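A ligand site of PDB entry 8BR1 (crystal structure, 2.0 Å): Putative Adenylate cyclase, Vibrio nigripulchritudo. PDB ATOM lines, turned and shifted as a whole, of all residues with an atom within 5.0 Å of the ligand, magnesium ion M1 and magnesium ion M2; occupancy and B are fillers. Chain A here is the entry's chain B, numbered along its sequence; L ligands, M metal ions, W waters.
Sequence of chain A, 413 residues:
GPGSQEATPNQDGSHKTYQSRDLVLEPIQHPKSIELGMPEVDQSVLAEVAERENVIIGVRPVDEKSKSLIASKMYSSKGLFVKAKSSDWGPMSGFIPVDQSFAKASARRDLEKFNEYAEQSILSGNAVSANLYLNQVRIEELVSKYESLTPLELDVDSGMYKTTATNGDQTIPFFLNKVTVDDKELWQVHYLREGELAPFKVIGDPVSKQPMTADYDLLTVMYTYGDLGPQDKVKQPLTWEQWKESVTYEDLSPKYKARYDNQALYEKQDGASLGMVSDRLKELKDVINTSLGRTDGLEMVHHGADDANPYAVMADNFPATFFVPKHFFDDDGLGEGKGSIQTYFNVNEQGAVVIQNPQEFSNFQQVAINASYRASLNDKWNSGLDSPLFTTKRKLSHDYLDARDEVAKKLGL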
ATOM      1  N   ARG A  60      -9.686 -29.329 -38.271  1.00  0.00           N
ATOM      2  CA  ARG A  60     -10.499 -30.453 -37.796  1.00  0.00           C
ATOM      3  C   ARG A  60     -12.027 -30.178 -37.988  1.00  0.00           C
ATOM      4  O   ARG A  60     -12.418 -29.030 -38.156  1.00  0.00           O
ATOM      5  CB  ARG A  60     -10.162 -30.726 -36.325  1.00  0.00           C
ATOM      6  CG  ARG A  60      -8.776 -31.382 -36.118  1.00  0.00           C
ATOM      7  CD  ARG A  60      -8.523 -31.666 -34.650  1.00  0.00           C
ATOM      8  NE  ARG A  60      -9.610 -32.485 -34.101  1.00  0.00           N
ATOM      9  CZ  ARG A  60     -10.283 -32.200 -32.994  1.00  0.00           C
ATOM     10  NH1 ARG A  60      -9.948 -31.158 -32.246  1.00  0.00           N
ATOM     11  NH2 ARG A  60     -11.303 -32.974 -32.623  1.00  0.00           N
ATOM     12  N   LYS A  78     -14.360 -21.826 -27.336  1.00  0.00           N
ATOM     13  CA  LYS A  78     -13.584 -22.499 -26.307  1.00  0.00           C
ATOM     14  C   LYS A  78     -12.093 -22.706 -26.649  1.00  0.00           C
ATOM     15  O   LYS A  78     -11.771 -23.410 -27.605  1.00  0.00           O
ATOM     16  CB  LYS A  78     -14.247 -23.862 -25.965  1.00  0.00           C
ATOM     17  CG  LYS A  78     -14.710 -24.652 -27.192  1.00  0.00           C
ATOM     18  CD  LYS A  78     -14.941 -26.135 -26.908  1.00  0.00           C
ATOM     19  CE  LYS A  78     -13.640 -26.897 -26.713  1.00  0.00           C
ATOM     20  NZ  LYS A  78     -13.874 -28.307 -26.280  1.00  0.00           N
ATOM     21  N   LEU A  80      -8.040 -23.733 -24.828  1.00  0.00           N
ATOM     22  CA  LEU A  80      -7.479 -24.805 -23.984  1.00  0.00           C
ATOM     23  C   LEU A  80      -7.986 -24.877 -22.551  1.00  0.00           C
ATOM     24  O   LEU A  80      -8.007 -25.959 -21.988  1.00  0.00           O
ATOM     25  CB  LEU A  80      -5.933 -24.755 -23.934  1.00  0.00           C
ATOM     26  CG  LEU A  80      -5.161 -25.104 -25.239  1.00  0.00           C
ATOM     27  CD1 LEU A  80      -3.760 -25.574 -24.910  1.00  0.00           C
ATOM     28  CD2 LEU A  80      -5.828 -26.226 -26.020  1.00  0.00           C
ATOM     29  N   VAL A  82     -10.963 -24.588 -21.581  1.00  0.00           N
ATOM     30  CA  VAL A  82     -12.278 -25.180 -21.603  1.00  0.00           C
ATOM     31  C   VAL A  82     -12.165 -26.463 -22.384  1.00  0.00           C
ATOM     32  O   VAL A  82     -12.348 -26.478 -23.613  1.00  0.00           O
ATOM     33  CB  VAL A  82     -13.330 -24.216 -22.224  1.00  0.00           C
ATOM     34  CG1 VAL A  82     -14.726 -24.845 -22.212  1.00  0.00           C
ATOM     35  CG2 VAL A  82     -13.323 -22.874 -21.513  1.00  0.00           C
ATOM     36  N   LYS A  83     -11.801 -27.535 -21.693  1.00  0.00           N
ATOM     37  CA  LYS A  83     -11.653 -28.846 -22.312  1.00  0.00           C
ATOM     38  C   LYS A  83     -12.972 -29.637 -22.419  1.00  0.00           C
ATOM     39  O   LYS A  83     -13.026 -30.633 -23.122  1.00  0.00           O
ATOM     40  CB  LYS A  83     -10.570 -29.671 -21.599  1.00  0.00           C
ATOM     41  CG  LYS A  83      -9.163 -29.064 -21.705  1.00  0.00           C
ATOM     42  CD  LYS A  83      -8.227 -29.797 -20.724  1.00  0.00           C
ATOM     43  CE  LYS A  83      -6.783 -29.371 -20.865  1.00  0.00           C
ATOM     44  NZ  LYS A  83      -6.599 -27.905 -20.561  1.00  0.00           N
ATOM     45  N   ALA A  84     -14.062 -29.171 -21.769  1.00  0.00           N
ATOM     46  CA  ALA A  84     -15.376 -29.797 -21.908  1.00  0.00           C
ATOM     47  C   ALA A  84     -15.808 -29.718 -23.383  1.00  0.00           C
ATOM     48  O   ALA A  84     -15.506 -28.720 -24.051  1.00  0.00           O
ATOM     49  CB  ALA A  84     -16.390 -29.067 -21.041  1.00  0.00           C
ATOM     50  N   LYS A  85     -16.418 -30.774 -23.908  1.00  0.00           N
ATOM     51  CA  LYS A  85     -16.780 -30.812 -25.320  1.00  0.00           C
ATOM     52  C   LYS A  85     -18.088 -30.130 -25.630  1.00  0.00           C
ATOM     53  O   LYS A  85     -18.993 -30.112 -24.799  1.00  0.00           O
ATOM     54  CB  LYS A  85     -16.808 -32.254 -25.842  1.00  0.00           C
ATOM     55  CG  LYS A  85     -15.470 -32.972 -25.634  1.00  0.00           C
ATOM     56  CD  LYS A  85     -14.715 -33.147 -26.925  1.00  0.00           C
ATOM     57  CE  LYS A  85     -13.494 -34.058 -26.805  1.00  0.00           C
ATOM     58  NZ  LYS A  85     -12.238 -33.253 -26.835  1.00  0.00           N
ATOM     59  N   SER A  86     -18.216 -29.655 -26.859  1.00  0.00           N
ATOM     60  CA  SER A  86     -19.475 -29.103 -27.330  1.00  0.00           C
ATOM     61  C   SER A  86     -20.444 -30.281 -27.557  1.00  0.00           C
ATOM     62  O   SER A  86     -20.039 -31.454 -27.601  1.00  0.00           O
ATOM     63  CB  SER A  86     -19.285 -28.335 -28.637  1.00  0.00           C
ATOM     64  OG  SER A  86     -18.987 -29.226 -29.694  1.00  0.00           O
ATOM     65  N   LYS A 104     -21.162 -34.211 -27.147  1.00  0.00           N
ATOM     66  CA  LYS A 104     -20.918 -35.185 -28.198  1.00  0.00           C
ATOM     67  C   LYS A 104     -20.396 -36.529 -27.573  1.00  0.00           C
ATOM     68  O   LYS A 104     -20.022 -36.559 -26.392  1.00  0.00           O
ATOM     69  CB  LYS A 104     -19.913 -34.620 -29.214  1.00  0.00           C
ATOM     70  CG  LYS A 104     -18.509 -34.469 -28.630  1.00  0.00           C
ATOM     71  CD  LYS A 104     -17.527 -33.958 -29.659  1.00  0.00           C
ATOM     72  CE  LYS A 104     -17.919 -32.619 -30.213  1.00  0.00           C
ATOM     73  NZ  LYS A 104     -16.925 -32.103 -31.190  1.00  0.00           N
ATOM     74  N   ALA A 214     -17.980 -24.128 -30.222  1.00  0.00           N
ATOM     75  CA  ALA A 214     -16.757 -24.833 -30.504  1.00  0.00           C
ATOM     76  C   ALA A 214     -15.766 -23.872 -31.239  1.00  0.00           C
ATOM     77  O   ALA A 214     -16.171 -22.894 -31.861  1.00  0.00           O
ATOM     78  CB  ALA A 214     -17.053 -26.031 -31.395  1.00  0.00           C
ATOM     79  N   ASP A 215     -14.500 -24.200 -31.224  1.00  0.00           N
ATOM     80  CA  ASP A 215     -13.442 -23.431 -31.888  1.00  0.00           C
ATOM     81  C   ASP A 215     -13.084 -24.064 -33.278  1.00  0.00           C
ATOM     82  O   ASP A 215     -13.685 -25.059 -33.704  1.00  0.00           O
ATOM     83  CB  ASP A 215     -12.207 -23.472 -30.947  1.00  0.00           C
ATOM     84  CG  ASP A 215     -11.678 -24.858 -30.591  1.00  0.00           C
ATOM     85  OD1 ASP A 215     -12.488 -25.786 -30.514  1.00  0.00           O
ATOM     86  OD2 ASP A 215     -10.459 -24.993 -30.357  1.00  0.00           O
ATOM     87  N   ASP A 217     -10.098 -26.024 -34.677  1.00  0.00           N
ATOM     88  CA  ASP A 217      -8.890 -26.682 -34.248  1.00  0.00           C
ATOM     89  C   ASP A 217      -8.046 -26.936 -35.471  1.00  0.00           C
ATOM     90  O   ASP A 217      -8.459 -27.706 -36.329  1.00  0.00           O
ATOM     91  CB  ASP A 217      -9.203 -28.012 -33.565  1.00  0.00           C
ATOM     92  CG  ASP A 217      -9.915 -27.803 -32.241  1.00  0.00           C
ATOM     93  OD1 ASP A 217      -9.221 -27.523 -31.241  1.00  0.00           O
ATOM     94  OD2 ASP A 217     -11.157 -27.929 -32.204  1.00  0.00           O
ATOM     95  N   LEU A 274      -1.703 -21.732 -25.430  1.00  0.00           N
ATOM     96  CA  LEU A 274      -1.445 -22.195 -26.790  1.00  0.00           C
ATOM     97  C   LEU A 274      -1.106 -23.684 -26.866  1.00  0.00           C
ATOM     98  O   LEU A 274      -1.242 -24.270 -27.922  1.00  0.00           O
ATOM     99  CB  LEU A 274      -0.269 -21.426 -27.440  1.00  0.00           C
ATOM    100  CG  LEU A 274      -0.367 -19.903 -27.492  1.00  0.00           C
ATOM    101  CD1 LEU A 274       0.949 -19.309 -27.871  1.00  0.00           C
ATOM    102  CD2 LEU A 274      -1.458 -19.447 -28.426  1.00  0.00           C
ATOM    103  N   GLY A 275      -0.584 -24.261 -25.784  1.00  0.00           N
ATOM    104  CA  GLY A 275      -0.156 -25.651 -25.795  1.00  0.00           C
ATOM    105  C   GLY A 275       1.182 -25.784 -26.492  1.00  0.00           C
ATOM    106  O   GLY A 275       2.004 -24.862 -26.427  1.00  0.00           O
ATOM    107  N   MET A 276       1.424 -26.908 -27.189  1.00  0.00           N
ATOM    108  CA  MET A 276       2.668 -27.161 -27.921  1.00  0.00           C
ATOM    109  C   MET A 276       2.520 -26.451 -29.261  1.00  0.00           C
ATOM    110  O   MET A 276       1.642 -26.797 -30.052  1.00  0.00           O
ATOM    111  CB  MET A 276       2.831 -28.659 -28.196  1.00  0.00           C
ATOM    112  CG  MET A 276       2.683 -29.529 -26.969  1.00  0.00           C
ATOM    113  SD  MET A 276       4.097 -29.347 -25.895  1.00  0.00           S
ATOM    114  CE  MET A 276       5.444 -29.891 -26.992  1.00  0.00           C
ATOM    115  N   HIS A 303      -5.106 -22.185 -30.146  1.00  0.00           N
ATOM    116  CA  HIS A 303      -3.929 -22.942 -29.728  1.00  0.00           C
ATOM    117  C   HIS A 303      -3.218 -23.638 -30.880  1.00  0.00           C
ATOM    118  O   HIS A 303      -3.634 -23.526 -32.022  1.00  0.00           O
ATOM    119  CB  HIS A 303      -4.385 -23.977 -28.666  1.00  0.00           C
ATOM    120  CG  HIS A 303      -5.566 -24.800 -29.098  1.00  0.00           C
ATOM    121  ND1 HIS A 303      -5.439 -25.840 -30.026  1.00  0.00           N
ATOM    122  CD2 HIS A 303      -6.864 -24.710 -28.725  1.00  0.00           C
ATOM    123  CE1 HIS A 303      -6.658 -26.343 -30.167  1.00  0.00           C
ATOM    124  NE2 HIS A 303      -7.548 -25.663 -29.430  1.00  0.00           N
ATOM    125  N   GLY A 304      -2.189 -24.406 -30.560  1.00  0.00           N
ATOM    126  CA  GLY A 304      -1.420 -25.177 -31.516  1.00  0.00           C
ATOM    127  C   GLY A 304      -2.233 -26.240 -32.231  1.00  0.00           C
ATOM    128  O   GLY A 304      -3.375 -26.584 -31.842  1.00  0.00           O
ATOM    129  N   ALA A 305      -1.631 -26.780 -33.290  1.00  0.00           N
ATOM    130  CA  ALA A 305      -2.249 -27.754 -34.145  1.00  0.00           C
ATOM    131  C   ALA A 305      -2.240 -29.148 -33.517  1.00  0.00           C
ATOM    132  O   ALA A 305      -1.415 -29.459 -32.654  1.00  0.00           O
ATOM    133  CB  ALA A 305      -1.559 -27.764 -35.518  1.00  0.00           C
ATOM    134  N   ASP A 306      -3.146 -30.014 -34.014  1.00  0.00           N
ATOM    135  CA  ASP A 306      -3.263 -31.374 -33.577  1.00  0.00           C
ATOM    136  C   ASP A 306      -2.012 -32.215 -33.847  1.00  0.00           C
ATOM    137  O   ASP A 306      -1.768 -33.188 -33.106  1.00  0.00           O
ATOM    138  CB  ASP A 306      -4.513 -31.980 -34.212  1.00  0.00           C
ATOM    139  CG  ASP A 306      -4.920 -33.243 -33.486  1.00  0.00           C
ATOM    140  OD1 ASP A 306      -5.473 -33.122 -32.354  1.00  0.00           O
ATOM    141  OD2 ASP A 306      -4.678 -34.321 -34.021  1.00  0.00           O
ATOM    142  N   ALA A 308       0.846 -31.596 -32.980  1.00  0.00           N
ATOM    143  CA  ALA A 308       1.642 -31.494 -31.753  1.00  0.00           C
ATOM    144  C   ALA A 308       0.835 -31.822 -30.491  1.00  0.00           C
ATOM    145  O   ALA A 308       1.296 -31.575 -29.383  1.00  0.00           O
ATOM    146  CB  ALA A 308       2.235 -30.084 -31.643  1.00  0.00           C
ATOM    147  N   ASN A 309      -0.369 -32.377 -30.626  1.00  0.00           N
ATOM    148  CA  ASN A 309      -1.255 -32.664 -29.509  1.00  0.00           C
ATOM    149  C   ASN A 309      -1.008 -34.062 -28.970  1.00  0.00           C
ATOM    150  O   ASN A 309      -1.261 -35.045 -29.664  1.00  0.00           O
ATOM    151  CB  ASN A 309      -2.694 -32.486 -29.987  1.00  0.00           C
ATOM    152  CG  ASN A 309      -3.756 -32.845 -28.992  1.00  0.00           C
ATOM    153  OD1 ASN A 309      -3.523 -32.984 -27.791  1.00  0.00           O
ATOM    154  ND2 ASN A 309      -4.974 -33.011 -29.496  1.00  0.00           N
ATOM    155  N   PRO A 310      -0.478 -34.173 -27.720  1.00  0.00           N
ATOM    156  CA  PRO A 310      -0.221 -35.506 -27.144  1.00  0.00           C
ATOM    157  C   PRO A 310      -1.467 -36.326 -26.873  1.00  0.00           C
ATOM    158  O   PRO A 310      -1.375 -37.519 -26.675  1.00  0.00           O
ATOM    159  CB  PRO A 310       0.503 -35.204 -25.811  1.00  0.00           C
ATOM    160  CG  PRO A 310       0.815 -33.753 -25.820  1.00  0.00           C
ATOM    161  CD  PRO A 310      -0.143 -33.097 -26.769  1.00  0.00           C
ATOM    162  N   TYR A 311      -2.616 -35.698 -26.858  1.00  0.00           N
ATOM    163  CA  TYR A 311      -3.888 -36.367 -26.617  1.00  0.00           C
ATOM    164  C   TYR A 311      -4.717 -36.476 -27.895  1.00  0.00           C
ATOM    165  O   TYR A 311      -5.937 -36.646 -27.793  1.00  0.00           O
ATOM    166  CB  TYR A 311      -4.673 -35.625 -25.512  1.00  0.00           C
ATOM    167  CG  TYR A 311      -3.824 -35.422 -24.275  1.00  0.00           C
ATOM    168  CD1 TYR A 311      -3.258 -36.502 -23.607  1.00  0.00           C
ATOM    169  CD2 TYR A 311      -3.418 -34.148 -23.892  1.00  0.00           C
ATOM    170  CE1 TYR A 311      -2.410 -36.318 -22.521  1.00  0.00           C
ATOM    171  CE2 TYR A 311      -2.563 -33.951 -22.807  1.00  0.00           C
ATOM    172  CZ  TYR A 311      -2.068 -35.035 -22.127  1.00  0.00           C
ATOM    173  OH  TYR A 311      -1.213 -34.848 -21.062  1.00  0.00           O
HETATM  174  P1  LIG L   1     -15.293 -29.296 -29.590  1.00  0.00           P
HETATM  175  O1  LIG L   1     -14.400 -28.149 -29.971  1.00  0.00           O
HETATM  176  O2  LIG L   1     -15.649 -29.287 -28.123  1.00  0.00           O
HETATM  177  O3  LIG L   1     -16.543 -29.393 -30.467  1.00  0.00           O
HETATM  178  P2  LIG L   1     -12.992 -30.944 -29.960  1.00  0.00           P
HETATM  179  O4  LIG L   1     -12.693 -32.392 -29.966  1.00  0.00           O
HETATM  180  O5  LIG L   1     -12.522 -30.062 -31.131  1.00  0.00           O
HETATM  181  O6  LIG L   1     -14.548 -30.682 -29.809  1.00  0.00           O
HETATM  182  P3  LIG L   1     -11.155 -29.383 -28.321  1.00  0.00           P
HETATM  183  O7  LIG L   1     -11.366 -28.202 -29.146  1.00  0.00           O
HETATM  184  O8  LIG L   1     -11.149 -29.112 -26.847  1.00  0.00           O
HETATM  185  O9  LIG L   1     -12.375 -30.365 -28.609  1.00  0.00           O
HETATM  186  O10 LIG L   1      -9.776 -30.165 -28.705  1.00  0.00           O
HETATM  187  C1  LIG L   1      -8.441 -29.666 -28.488  1.00  0.00           C
HETATM  188  C2  LIG L   1      -7.913 -30.250 -27.218  1.00  0.00           C
HETATM  189  O11 LIG L   1      -6.729 -31.015 -27.519  1.00  0.00           O
HETATM  190  C3  LIG L   1      -7.468 -29.176 -26.231  1.00  0.00           C
HETATM  191  C4  LIG L   1      -6.222 -29.765 -25.582  1.00  0.00           C
HETATM  192  O12 LIG L   1      -6.613 -30.559 -24.456  1.00  0.00           O
HETATM  193  C5  LIG L   1      -5.626 -30.614 -26.718  1.00  0.00           C
HETATM  194  N1  LIG L   1      -4.676 -29.926 -27.610  1.00  0.00           N
HETATM  195  C6  LIG L   1      -4.907 -29.593 -28.918  1.00  0.00           C
HETATM  196  N2  LIG L   1      -3.861 -29.093 -29.533  1.00  0.00           N
HETATM  197  C7  LIG L   1      -2.881 -29.081 -28.557  1.00  0.00           C
HETATM  198  C8  LIG L   1      -1.537 -28.665 -28.578  1.00  0.00           C
HETATM  199  N3  LIG L   1      -0.907 -28.224 -29.680  1.00  0.00           N
HETATM  200  N4  LIG L   1      -0.824 -28.769 -27.427  1.00  0.00           N
HETATM  201  C9  LIG L   1      -1.425 -29.273 -26.344  1.00  0.00           C
HETATM  202  N5  LIG L   1      -2.680 -29.715 -26.216  1.00  0.00           N
HETATM  203  C10 LIG L   1      -3.360 -29.582 -27.361  1.00  0.00           C
HETATM  204 MG    MG M   1      -9.593 -26.588 -29.466  1.00  0.00          MG
HETATM  205 MG    MG M   2     -12.784 -27.863 -31.003  1.00  0.00          MG
HETATM  206  O   HOH W   1      -9.967 -27.108 -25.529  1.00  0.00           O
HETATM  207  O   HOH W   2     -14.033 -27.851 -32.883  1.00  0.00           O
HETATM  208  O   HOH W   3     -16.433 -28.858 -33.061  1.00  0.00           O
HETATM  209  O   HOH W   4     -12.984 -30.554 -33.999  1.00  0.00           O
HETATM  210  O   HOH W   5     -11.368 -31.365 -25.197  1.00  0.00           O
HETATM  211  O   HOH W   6      -9.993 -25.527 -27.748  1.00  0.00           O
HETATM  212  O   HOH W   7     -14.329 -33.995 -30.971  1.00  0.00           O
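NZ of Lys 85 is in salt-bridge range of O4 of the ligand, 3.3 Å away. The backbone carbonyl oxygen (O) of Ala 305 sits at hydrogen-bond distance from a nitrogen (N3) of the ligand (3.3 Å). The side-chain amino group of Lys 78 is in salt-bridge range of an oxygen (O2) of the ligand. N of Met 276 is in hydrogen-bond range of N4 of the ligand (2.9 Å). N of Ser 86 sits at hydrogen-bond distance from O2 of the ligand (2.9 Å). The backbone carbonyl oxygen (O) of Met 276 sits at hydrogen-bond distance from a nitrogen (N3) of the ligand. OG of Ser 86 is in hydrogen-bond range of O3 of the ligand (2.6 Å). The side-chain amide nitrogen of Asn 309 is in hydrogen-bond range of an oxygen (O11) of the ligand. O4 of the ligand lies within salt-bridge range of NH2 of Arg 60, at 3.1 Å. The side-chain amino group (NZ) of Lys 104 is in salt-bridge range of an oxygen (O3) of the ligand, 2.8 Å away.
O of Asp 217 lies within hydrogen-bond range of N of Arg 60, 2.8 Å away. The side-chain amino group of Lys 83 is in hydrogen-bond range of the backbone carbonyl oxygen of Leu 80, 2.8 Å away. NZ of Lys 78 sits at hydrogen-bond distance from O of Ala 84. N of Tyr 311 lies within hydrogen-bond range of OD1 of Asn 309 (3.0 Å). The backbone carbonyl oxygen of Ser 86 sits at hydrogen-bond distance from the backbone NH of Lys 104 (3.0 Å). OD1 of Asp 306 lies within hydrogen-bond range of ND2 of Asn 309 (2.9 Å). The backbone NH of Gly 304 is in hydrogen-bond range of the backbone carbonyl oxygen of Leu 274, at 2.8 Å.
The backbone carbonyl oxygen (O) of Gly 304 sits close to a nitrogen (N2) of the ligand (3.4 Å). Leu 80 touches the ligand (CD2 to C3, 3.4 Å). CE of Lys 83 touches O12 of the ligand, 3.8 Å away. CB of Ala 214 touches O3 of the ligand (3.5 Å). Gly 275 touches the ligand. Within 4 Å of the ligand: Arg 60, Lys 78, Leu 80, Lys 83, Lys 85, Ser 86, Lys 104, Ala 214, Asp 215, Asp 217, Gly 275, Met 276, His 303, Gly 304, Ala 305 and Asn 309.
Of the 23 residues printed, 3 come within 4 Å of magnesium ion M1.
Two residues have an atom within 4 Å of magnesium ion M2: Asp 215 and Asp 217.
Magnesium ion M1 is bound by the side-chain carboxylate (OD2) of Asp 215 (2.0 Å), the side-chain carboxylate (OD1) of Asp 217 (2.0 Å), water W6 (2.1 Å), a ring nitrogen (NE2) of His 303 (2.2 Å) and an oxygen (O7) of the ligand (2.4 Å). Magnesium ion M1 has five donor atoms within binding distance.
Magnesium ion M2 is bound by O1 of the ligand (1.9 Å), OD2 of Asp 217 (2.0 Å), OD1 of Asp 215 (2.2 Å), O5 of the ligand (2.2 Å), water W2 (2.3 Å) and O7 of the ligand (2.4 Å).
Water W7 bridges O4 of the ligand (2.5 Å) and NZ of Lys 104 (3.2 Å). Water W1 lies within hydrogen-bond range of O8 of the ligand and O of Val 82. Water W5 lies within hydrogen-bond range of the side-chain amino group (NZ) of Lys 85 (2.6 Å), the backbone carbonyl oxygen (O) of Lys 83 (2.8 Å) and an oxygen (O8) of the ligand (2.8 Å).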
